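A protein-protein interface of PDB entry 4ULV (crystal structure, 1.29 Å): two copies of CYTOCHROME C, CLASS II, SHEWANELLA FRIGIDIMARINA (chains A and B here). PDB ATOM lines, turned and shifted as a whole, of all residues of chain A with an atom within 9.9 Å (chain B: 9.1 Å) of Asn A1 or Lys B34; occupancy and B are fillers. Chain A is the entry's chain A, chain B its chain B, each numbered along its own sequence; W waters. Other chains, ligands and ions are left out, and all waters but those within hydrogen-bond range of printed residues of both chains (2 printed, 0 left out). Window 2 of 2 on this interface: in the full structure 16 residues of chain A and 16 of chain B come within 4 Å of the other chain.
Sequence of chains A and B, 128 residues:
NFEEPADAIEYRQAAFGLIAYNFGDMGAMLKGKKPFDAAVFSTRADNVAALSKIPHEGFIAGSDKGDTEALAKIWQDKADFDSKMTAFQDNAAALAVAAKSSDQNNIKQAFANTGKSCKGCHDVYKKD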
ATOM      1  N   ASN A   1       5.246  -4.544  11.314  1.00  0.00           N
ATOM      2  CA  ASN A   1       4.476  -3.256  10.919  1.00  0.00           C
ATOM      3  C   ASN A   1       3.915  -3.157   9.466  1.00  0.00           C
ATOM      4  O   ASN A   1       3.277  -2.163   9.068  1.00  0.00           O
ATOM      5  CB  ASN A   1       5.315  -2.023  11.211  1.00  0.00           C
ATOM      6  CG  ASN A   1       4.872  -1.300  12.465  1.00  0.00           C
ATOM      7  OD1 ASN A   1       4.553  -1.936  13.487  1.00  0.00           O
ATOM      8  ND2 ASN A   1       4.879   0.056  12.408  1.00  0.00           N
ATOM      9  N   PHE A   2       4.066  -4.229   8.721  1.00  0.00           N
ATOM     10  CA  PHE A   2       3.646  -4.260   7.328  1.00  0.00           C
ATOM     11  C   PHE A   2       2.168  -4.463   7.208  1.00  0.00           C
ATOM     12  O   PHE A   2       1.587  -5.369   7.749  1.00  0.00           O
ATOM     13  CB  PHE A   2       4.424  -5.324   6.603  1.00  0.00           C
ATOM     14  CG  PHE A   2       5.919  -5.105   6.655  1.00  0.00           C
ATOM     15  CD1 PHE A   2       6.500  -4.000   6.043  1.00  0.00           C
ATOM     16  CD2 PHE A   2       6.727  -6.017   7.315  1.00  0.00           C
ATOM     17  CE1 PHE A   2       7.873  -3.812   6.149  1.00  0.00           C
ATOM     18  CE2 PHE A   2       8.096  -5.840   7.395  1.00  0.00           C
ATOM     19  CZ  PHE A   2       8.662  -4.753   6.780  1.00  0.00           C
ATOM     20  N   GLU A   3       1.600  -3.560   6.435  1.00  0.00           N
ATOM     21  CA  GLU A   3       0.173  -3.468   6.237  1.00  0.00           C
ATOM     22  C   GLU A   3      -0.253  -4.716   5.447  1.00  0.00           C
ATOM     23  O   GLU A   3      -1.265  -5.274   5.642  1.00  0.00           O
ATOM     24  CB  GLU A   3       0.007  -2.216   5.351  1.00  0.00           C
ATOM     25  CG  GLU A   3       0.148  -0.906   6.117  1.00  0.00           C
ATOM     26  CD  GLU A   3       1.183   0.032   5.512  1.00  0.00           C
ATOM     27  OE2 GLU A   3       0.876   1.242   5.357  1.00  0.00           O
ATOM     28  N   GLU A   4       0.575  -5.104   4.470  1.00  0.00           N
ATOM     29  CA  GLU A   4       0.373  -6.361   3.675  1.00  0.00           C
ATOM     30  C   GLU A   4       1.699  -7.056   3.385  1.00  0.00           C
ATOM     31  O   GLU A   4       2.694  -6.385   3.385  1.00  0.00           O
ATOM     32  CB  GLU A   4      -0.261  -6.056   2.301  1.00  0.00           C
ATOM     33  CG  GLU A   4      -1.430  -5.068   2.310  1.00  0.00           C
ATOM     34  N   PRO A   5       1.712  -8.377   3.066  1.00  0.00           N
ATOM     35  CA  PRO A   5       3.021  -9.029   2.834  1.00  0.00           C
ATOM     36  C   PRO A   5       3.793  -8.477   1.667  1.00  0.00           C
ATOM     37  O   PRO A   5       5.040  -8.518   1.662  1.00  0.00           O
ATOM     38  CB  PRO A   5       2.668 -10.485   2.544  1.00  0.00           C
ATOM     39  CG  PRO A   5       1.276 -10.675   3.025  1.00  0.00           C
ATOM     40  CD  PRO A   5       0.595  -9.341   3.092  1.00  0.00           C
ATOM     41  N   ASP A   7       4.221  -5.534   1.081  1.00  0.00           N
ATOM     42  CA  ASP A   7       4.984  -4.427   1.642  1.00  0.00           C
ATOM     43  C   ASP A   7       6.331  -4.897   2.217  1.00  0.00           C
ATOM     44  O   ASP A   7       7.293  -4.176   2.114  1.00  0.00           O
ATOM     45  CB  ASP A   7       4.152  -3.652   2.677  1.00  0.00           C
ATOM     46  CG  ASP A   7       2.891  -3.006   2.080  1.00  0.00           C
ATOM     47  OD1 ASP A   7       2.875  -2.547   0.933  1.00  0.00           O
ATOM     48  OD2 ASP A   7       1.881  -2.937   2.774  1.00  0.00           O
ATOM     49  N   ALA A   8       6.295  -6.043   2.869  1.00  0.00           N
ATOM     50  CA  ALA A   8       7.509  -6.596   3.489  1.00  0.00           C
ATOM     51  C   ALA A   8       8.493  -6.920   2.401  1.00  0.00           C
ATOM     52  O   ALA A   8       9.718  -6.739   2.537  1.00  0.00           O
ATOM     53  CB  ALA A   8       7.141  -7.839   4.258  1.00  0.00           C
ATOM     54  N   TYR A  11       9.911  -3.702   0.942  1.00  0.00           N
ATOM     55  CA  TYR A  11      10.840  -3.115   1.922  1.00  0.00           C
ATOM     56  C   TYR A  11      12.221  -3.795   1.806  1.00  0.00           C
ATOM     57  O   TYR A  11      13.265  -3.087   1.676  1.00  0.00           O
ATOM     58  CB  TYR A  11      10.238  -3.270   3.292  1.00  0.00           C
ATOM     59  CG  TYR A  11      11.027  -2.648   4.436  1.00  0.00           C
ATOM     60  CD1 TYR A  11      10.838  -1.329   4.793  1.00  0.00           C
ATOM     61  CD2 TYR A  11      11.942  -3.404   5.155  1.00  0.00           C
ATOM     62  CE1 TYR A  11      11.529  -0.773   5.855  1.00  0.00           C
ATOM     63  CE2 TYR A  11      12.670  -2.847   6.188  1.00  0.00           C
ATOM     64  CZ  TYR A  11      12.455  -1.526   6.523  1.00  0.00           C
ATOM     65  OH  TYR A  11      13.120  -0.888   7.563  1.00  0.00           O
ATOM     66  N   GLU A  57      14.105  -7.383   8.646  1.00  0.00           N
ATOM     67  CA  GLU A  57      12.741  -7.135   9.128  1.00  0.00           C
ATOM     68  C   GLU A  57      11.678  -7.554   8.096  1.00  0.00           C
ATOM     69  O   GLU A  57      10.569  -7.951   8.498  1.00  0.00           O
ATOM     70  CB  GLU A  57      12.595  -5.674   9.469  1.00  0.00           C
ATOM     71  CG  GLU A  57      11.232  -5.351  10.126  1.00  0.00           C
ATOM     72  CD  GLU A  57      11.048  -3.940  10.589  1.00  0.00           C
ATOM     73  OE1 GLU A  57      12.027  -3.134  10.479  1.00  0.00           O
ATOM     74  OE2 GLU A  57       9.952  -3.663  11.157  1.00  0.00           O
ATOM     75  N   GLY A  58      12.009  -7.451   6.820  1.00  0.00           N
ATOM     76  CA  GLY A  58      11.042  -7.838   5.800  1.00  0.00           C
ATOM     77  C   GLY A  58      10.800  -9.327   5.620  1.00  0.00           C
ATOM     78  O   GLY A  58       9.872  -9.686   4.878  1.00  0.00           O
ATOM     79  N   ILE A  60       9.212 -11.868   6.698  1.00  0.00           N
ATOM     80  CA  ILE A  60       8.097 -12.345   7.498  1.00  0.00           C
ATOM     81  C   ILE A  60       7.609 -13.698   6.997  1.00  0.00           C
ATOM     82  O   ILE A  60       7.701 -14.019   5.762  1.00  0.00           O
ATOM     83  CB  ILE A  60       6.975 -11.269   7.591  1.00  0.00           C
ATOM     84  CG1 ILE A  60       6.296 -11.092   6.210  1.00  0.00           C
ATOM     85  CG2 ILE A  60       7.586  -9.957   8.078  1.00  0.00           C
ATOM     86  CD1 ILE A  60       5.093 -10.166   6.326  1.00  0.00           C
ATOM     87  N   ALA B  20      10.307   6.531   5.515  1.00  0.00           N
ATOM     88  CA  ALA B  20       8.909   6.719   5.973  1.00  0.00           C
ATOM     89  C   ALA B  20       8.488   5.585   6.885  1.00  0.00           C
ATOM     90  O   ALA B  20       7.799   5.782   7.894  1.00  0.00           O
ATOM     91  CB  ALA B  20       7.997   6.860   4.781  1.00  0.00           C
ATOM     92  N   TYR B  21       8.907   4.370   6.560  1.00  0.00           N
ATOM     93  CA  TYR B  21       8.511   3.231   7.365  1.00  0.00           C
ATOM     94  C   TYR B  21       9.096   3.343   8.786  1.00  0.00           C
ATOM     95  O   TYR B  21       8.407   3.159   9.812  1.00  0.00           O
ATOM     96  CB  TYR B  21       8.970   1.928   6.716  1.00  0.00           C
ATOM     97  CG  TYR B  21       8.699   0.687   7.519  1.00  0.00           C
ATOM     98  CD1 TYR B  21       7.511   0.006   7.402  1.00  0.00           C
ATOM     99  CD2 TYR B  21       9.661   0.163   8.410  1.00  0.00           C
ATOM    100  CE1 TYR B  21       7.245  -1.125   8.106  1.00  0.00           C
ATOM    101  CE2 TYR B  21       9.389  -0.942   9.143  1.00  0.00           C
ATOM    102  CZ  TYR B  21       8.183  -1.617   8.982  1.00  0.00           C
ATOM    103  OH  TYR B  21       7.874  -2.741   9.695  1.00  0.00           O
ATOM    104  N   ASN B  22      10.389   3.660   8.869  1.00  0.00           N
ATOM    105  CA  ASN B  22      11.061   3.778  10.131  1.00  0.00           C
ATOM    106  C   ASN B  22      10.581   5.022  10.900  1.00  0.00           C
ATOM    107  O   ASN B  22      10.367   4.967  12.138  1.00  0.00           O
ATOM    108  CB  ASN B  22      12.586   3.766   9.931  1.00  0.00           C
ATOM    109  CG  ASN B  22      13.089   2.371   9.654  1.00  0.00           C
ATOM    110  OD1 ASN B  22      13.296   1.584  10.589  1.00  0.00           O
ATOM    111  ND2 ASN B  22      13.150   1.997   8.339  1.00  0.00           N
ATOM    112  N   PHE B  23      10.445   6.126  10.205  1.00  0.00           N
ATOM    113  CA  PHE B  23       9.951   7.362  10.846  1.00  0.00           C
ATOM    114  C   PHE B  23       8.518   7.165  11.355  1.00  0.00           C
ATOM    115  O   PHE B  23       8.190   7.655  12.461  1.00  0.00           O
ATOM    116  CB  PHE B  23      10.035   8.536   9.867  1.00  0.00           C
ATOM    117  CG  PHE B  23       9.851   9.889  10.509  1.00  0.00           C
ATOM    118  CD1 PHE B  23      10.843  10.425  11.280  1.00  0.00           C
ATOM    119  CD2 PHE B  23       8.722  10.613  10.254  1.00  0.00           C
ATOM    120  CE1 PHE B  23      10.684  11.651  11.820  1.00  0.00           C
ATOM    121  CE2 PHE B  23       8.537  11.831  10.860  1.00  0.00           C
ATOM    122  CZ  PHE B  23       9.514  12.348  11.631  1.00  0.00           C
ATOM    123  N   GLY B  24       7.700   6.480  10.588  1.00  0.00           N
ATOM    124  CA  GLY B  24       6.326   6.239  10.987  1.00  0.00           C
ATOM    125  C   GLY B  24       6.211   5.407  12.244  1.00  0.00           C
ATOM    126  O   GLY B  24       5.309   5.615  13.031  1.00  0.00           O
ATOM    127  N   ASP B  25       7.158   4.488  12.466  1.00  0.00           N
ATOM    128  CA  ASP B  25       7.095   3.694  13.663  1.00  0.00           C
ATOM    129  C   ASP B  25       7.418   4.540  14.920  1.00  0.00           C
ATOM    130  O   ASP B  25       6.751   4.370  15.970  1.00  0.00           O
ATOM    131  CB  ASP B  25       8.037   2.479  13.566  1.00  0.00           C
ATOM    132  CG  ASP B  25       7.721   1.405  14.579  1.00  0.00           C
ATOM    133  OD1 ASP B  25       6.518   1.098  14.742  1.00  0.00           O
ATOM    134  OD2 ASP B  25       8.646   0.876  15.235  1.00  0.00           O
ATOM    135  N   MET B  26       8.352   5.487  14.795  1.00  0.00           N
ATOM    136  CA  MET B  26       8.580   6.422  15.878  1.00  0.00           C
ATOM    137  C   MET B  26       7.304   7.245  16.129  1.00  0.00           C
ATOM    138  O   MET B  26       6.922   7.502  17.283  1.00  0.00           O
ATOM    139  CB  MET B  26       9.724   7.363  15.583  1.00  0.00           C
ATOM    140  CG  MET B  26      11.092   6.662  15.664  1.00  0.00           C
ATOM    141  SD  MET B  26      12.518   7.750  15.513  1.00  0.00           S
ATOM    142  CE  MET B  26      12.556   7.814  13.777  1.00  0.00           C
ATOM    143  N   GLY B  27       6.706   7.705  15.026  1.00  0.00           N
ATOM    144  CA  GLY B  27       5.438   8.438  15.126  1.00  0.00           C
ATOM    145  C   GLY B  27       4.367   7.686  15.881  1.00  0.00           C
ATOM    146  O   GLY B  27       3.642   8.262  16.715  1.00  0.00           O
ATOM    147  N   ALA B  28       4.219   6.427  15.612  1.00  0.00           N
ATOM    148  CA  ALA B  28       3.218   5.588  16.236  1.00  0.00           C
ATOM    149  C   ALA B  28       3.448   5.547  17.712  1.00  0.00           C
ATOM    150  O   ALA B  28       2.463   5.574  18.500  1.00  0.00           O
ATOM    151  CB  ALA B  28       3.229   4.216  15.626  1.00  0.00           C
ATOM    152  N   MET B  29       4.733   5.427  18.095  1.00  0.00           N
ATOM    153  CA  MET B  29       5.044   5.375  19.542  1.00  0.00           C
ATOM    154  C   MET B  29       4.714   6.728  20.183  1.00  0.00           C
ATOM    155  O   MET B  29       4.133   6.782  21.267  1.00  0.00           O
ATOM    156  CB  MET B  29       6.507   4.970  19.781  1.00  0.00           C
ATOM    157  CG  MET B  29       6.729   3.540  19.367  1.00  0.00           C
ATOM    158  SD  MET B  29       8.378   3.005  19.743  1.00  0.00           S
ATOM    159  CE  MET B  29       8.405   1.447  18.928  1.00  0.00           C
ATOM    160  N   LEU B  30       5.049   7.833  19.529  1.00  0.00           N
ATOM    161  CA  LEU B  30       4.803   9.143  20.190  1.00  0.00           C
ATOM    162  C   LEU B  30       3.343   9.602  20.169  1.00  0.00           C
ATOM    163  O   LEU B  30       2.954  10.344  21.033  1.00  0.00           O
ATOM    164  CB  LEU B  30       5.693  10.216  19.566  1.00  0.00           C
ATOM    165  CG  LEU B  30       7.206   9.922  19.671  1.00  0.00           C
ATOM    166  CD1 LEU B  30       7.965  10.912  18.833  1.00  0.00           C
ATOM    167  CD2 LEU B  30       7.742   9.858  21.111  1.00  0.00           C
ATOM    168  N   LYS B  31       2.570   9.113  19.202  1.00  0.00           N
ATOM    169  CA  LYS B  31       1.138   9.491  18.996  1.00  0.00           C
ATOM    170  C   LYS B  31       0.266   8.666  19.933  1.00  0.00           C
ATOM    171  O   LYS B  31      -0.899   9.000  20.132  1.00  0.00           O
ATOM    172  CB  LYS B  31       0.717   9.121  17.547  1.00  0.00           C
ATOM    173  CG  LYS B  31       0.903  10.177  16.501  1.00  0.00           C
ATOM    174  CD  LYS B  31       0.252   9.704  15.213  1.00  0.00           C
ATOM    175  CE  LYS B  31       0.808  10.467  14.034  1.00  0.00           C
ATOM    176  NZ  LYS B  31      -0.038  10.296  12.845  1.00  0.00           N
ATOM    177  N   GLY B  32       0.834   7.565  20.449  1.00  0.00           N
ATOM    178  CA  GLY B  32       0.142   6.601  21.285  1.00  0.00           C
ATOM    179  C   GLY B  32      -0.593   5.477  20.613  1.00  0.00           C
ATOM    180  O   GLY B  32      -1.364   4.752  21.272  1.00  0.00           O
ATOM    181  N   LYS B  33      -0.295   5.268  19.334  1.00  0.00           N
ATOM    182  CA  LYS B  33      -0.869   4.112  18.617  1.00  0.00           C
ATOM    183  C   LYS B  33      -0.251   2.813  19.171  1.00  0.00           C
ATOM    184  O   LYS B  33      -0.939   1.795  19.250  1.00  0.00           O
ATOM    185  CB  LYS B  33      -0.709   4.215  17.097  1.00  0.00           C
ATOM    186  CG  LYS B  33      -1.114   2.932  16.396  1.00  0.00           C
ATOM    187  CD  LYS B  33      -1.083   3.079  14.895  1.00  0.00           C
ATOM    188  CE  LYS B  33      -1.615   1.804  14.295  1.00  0.00           C
ATOM    189  NZ  LYS B  33      -1.870   1.960  12.845  1.00  0.00           N
ATOM    190  N   LYS B  34       1.003   2.870  19.614  1.00  0.00           N
ATOM    191  CA  LYS B  34       1.649   1.706  20.300  1.00  0.00           C
ATOM    192  C   LYS B  34       2.519   2.250  21.429  1.00  0.00           C
ATOM    193  O   LYS B  34       2.873   3.430  21.393  1.00  0.00           O
ATOM    194  CB  LYS B  34       2.441   0.876  19.306  1.00  0.00           C
ATOM    195  CG  LYS B  34       3.575   1.654  18.646  1.00  0.00           C
ATOM    196  CD  LYS B  34       4.108   1.060  17.352  1.00  0.00           C
ATOM    197  CE  LYS B  34       4.540  -0.346  17.541  1.00  0.00           C
ATOM    198  NZ  LYS B  34       4.928  -0.895  16.199  1.00  0.00           N
ATOM    199  N   PRO B  35       2.778   1.438  22.480  1.00  0.00           N
ATOM    200  CA  PRO B  35       3.558   1.983  23.618  1.00  0.00           C
ATOM    201  C   PRO B  35       4.974   2.357  23.185  1.00  0.00           C
ATOM    202  O   PRO B  35       5.575   1.716  22.320  1.00  0.00           O
ATOM    203  CB  PRO B  35       3.586   0.834  24.660  1.00  0.00           C
ATOM    204  CG  PRO B  35       2.925  -0.354  24.001  1.00  0.00           C
ATOM    205  CD  PRO B  35       2.231   0.086  22.730  1.00  0.00           C
ATOM    206  N   PHE B  36       5.517   3.371  23.840  1.00  0.00           N
ATOM    207  CA  PHE B  36       6.857   3.717  23.616  1.00  0.00           C
ATOM    208  C   PHE B  36       7.775   2.585  24.109  1.00  0.00           C
ATOM    209  O   PHE B  36       7.645   2.114  25.263  1.00  0.00           O
ATOM    210  CB  PHE B  36       7.144   5.021  24.329  1.00  0.00           C
ATOM    211  CG  PHE B  36       8.534   5.516  24.102  1.00  0.00           C
ATOM    212  CD1 PHE B  36       9.603   5.131  24.922  1.00  0.00           C
ATOM    213  CD2 PHE B  36       8.790   6.334  23.005  1.00  0.00           C
ATOM    214  CE1 PHE B  36      10.878   5.583  24.660  1.00  0.00           C
ATOM    215  CE2 PHE B  36      10.060   6.768  22.749  1.00  0.00           C
ATOM    216  CZ  PHE B  36      11.095   6.420  23.594  1.00  0.00           C
ATOM    217  N   ASP B  37       8.694   2.171  23.224  1.00  0.00           N
ATOM    218  CA  ASP B  37       9.666   1.090  23.495  1.00  0.00           C
ATOM    219  C   ASP B  37      11.012   1.714  23.171  1.00  0.00           C
ATOM    220  O   ASP B  37      11.285   1.998  22.011  1.00  0.00           O
ATOM    221  CB  ASP B  37       9.394  -0.110  22.575  1.00  0.00           C
ATOM    222  CG  ASP B  37      10.380  -1.265  22.811  1.00  0.00           C
ATOM    223  OD1 ASP B  37      11.582  -1.044  22.939  1.00  0.00           O
ATOM    224  OD2 ASP B  37       9.931  -2.386  22.925  1.00  0.00           O
ATOM    225  N   VAL B  40      13.413  -0.231  20.546  1.00  0.00           N
ATOM    226  CA  VAL B  40      12.990  -0.177  19.189  1.00  0.00           C
ATOM    227  C   VAL B  40      13.078   1.264  18.650  1.00  0.00           C
ATOM    228  O   VAL B  40      13.532   1.529  17.542  1.00  0.00           O
ATOM    229  CB  VAL B  40      11.575  -0.789  19.019  1.00  0.00           C
ATOM    230  CG1 VAL B  40      11.041  -0.531  17.606  1.00  0.00           C
ATOM    231  CG2 VAL B  40      11.617  -2.287  19.320  1.00  0.00           C
ATOM    232  N   PHE B  41      12.682   2.204  19.498  1.00  0.00           N
ATOM    233  CA  PHE B  41      12.711   3.617  19.104  1.00  0.00           C
ATOM    234  C   PHE B  41      14.136   4.038  18.680  1.00  0.00           C
ATOM    235  O   PHE B  41      14.341   4.729  17.670  1.00  0.00           O
ATOM    236  CB  PHE B  41      12.108   4.538  20.176  1.00  0.00           C
ATOM    237  CG  PHE B  41      11.822   5.935  19.695  1.00  0.00           C
ATOM    238  CD1 PHE B  41      12.849   6.878  19.614  1.00  0.00           C
ATOM    239  CD2 PHE B  41      10.527   6.341  19.382  1.00  0.00           C
ATOM    240  CE1 PHE B  41      12.577   8.202  19.222  1.00  0.00           C
ATOM    241  CE2 PHE B  41      10.282   7.614  18.929  1.00  0.00           C
ATOM    242  CZ  PHE B  41      11.256   8.557  18.868  1.00  0.00           C
ATOM    243  N   ARG B  44      14.938   2.652  15.297  1.00  0.00           N
ATOM    244  CA  ARG B  44      14.286   3.437  14.258  1.00  0.00           C
ATOM    245  C   ARG B  44      14.949   4.769  14.009  1.00  0.00           C
ATOM    246  O   ARG B  44      15.118   5.186  12.888  1.00  0.00           O
ATOM    247  CB  ARG B  44      12.830   3.705  14.620  1.00  0.00           C
ATOM    248  CG  ARG B  44      11.960   2.483  14.803  1.00  0.00           C
ATOM    249  CD  ARG B  44      11.928   1.585  13.568  1.00  0.00           C
ATOM    250  NE  ARG B  44      11.073   0.421  13.707  1.00  0.00           N
ATOM    251  CZ  ARG B  44      11.062  -0.625  12.877  1.00  0.00           C
ATOM    252  NH1 ARG B  44      11.885  -0.664  11.835  1.00  0.00           N
ATOM    253  NH2 ARG B  44      10.265  -1.633  13.122  1.00  0.00           N
HETATM  254  O   HOH W   1       5.845   2.083  10.030  1.00  0.00           O
HETATM  255  O   HOH W   2       7.907  -5.576  11.565  1.00  0.00           O
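The side-chain carboxylate (OD1) of Asp B25 lies within hydrogen-bond range of the side-chain amide nitrogen (ND2) of Asn A1. OD1 of Asn A1 is in hydrogen-bond range of NZ of Lys B34 (2.9 Å). The side-chain hydroxyl of Tyr A11 lies within hydrogen-bond range of the side-chain amide nitrogen of Asn B22, at 3.0 Å. OE2 of Glu A57 lies within hydrogen-bond range of OH of Tyr B21 (2.7 Å). OE1 of Glu A57 lies within salt-bridge range of NH1 of Arg B44, at 2.8 Å.
Water W1 bridges the backbone carbonyl oxygen (O) of Tyr B21 and the side-chain amide nitrogen (ND2) of Asn A1. Water W2 lies within hydrogen-bond range of the side-chain carboxylate of Glu A57, the backbone NH of Asn A1 and the side-chain hydroxyl of Tyr B21.
Among the printed residues, pairs that only touch across the chains: Asn A1 with Tyr B21 (3.1 Å), Tyr A11 with Tyr B21 (3.3 Å) and Phe A2 with Tyr B21 (3.4 Å).
No position is printed for both chains.
Hydrophobic or aromatic side chains of chain A within 4 Å of the printed part of chain B: Phe A2 and Tyr A11. Along chain B the printed residues that touch a printed residue of chain A span positions 21 to 44. Among the printed residues, Asp or Glu carboxylates within 4 Å of a Lys or Arg side-chain nitrogen of the other chain: Glu A57 with Arg B44 (2.8 Å).
Asn A1 touches just these residues of chain B: Tyr B21, Asp B25 and Lys B34. Of chain A, only Asn A1 comes within 4 Å of Lys B34. No residue of chain A comes within 4 Å of Ala B28. No residue of chain A comes within 4 Å of Met B29. No residue of chain A comes within 4 Å of Gly B32. No residue of chain A comes within 4 Å of Pro B35. Printed residues of chain A within 4 Å of Arg B44: Glu A57. Printed residues of chain A within 4 Å of Asn B22: Tyr A11. Of the printed residues of chain A, Tyr B21 touches Asn A1, Phe A2, Tyr A11 and Glu A57. Printed residues of chain B within 4 Å of Phe A2: Tyr B21 (3.4 Å). Phe B41 touches none of the printed residues of chain A. Gly A58 touches none of the printed residues of chain B. The nearest residue of chain B that does not touch Asn A1 is Arg B44 (5.3 Å). The nearest residue of chain A that does not touch Lys B34 is Glu A57 (7.6 Å).
The side-chain amide oxygen (OD1) of Asn B22 lies within hydrogen-bond range of the guanidinium group (NH1) of Arg B44 (2.9 Å). OD1 of Asp B25 is in salt-bridge range of NZ of Lys B34 (2.9 Å). The side-chain carboxylate of Asp B25 is in salt-bridge range of the guanidinium group of Arg B44 (2.9 Å). The backbone carbonyl oxygen (O) of Ala B28 is in hydrogen-bond range of the backbone NH (N) of Lys B34 (3.3 Å).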
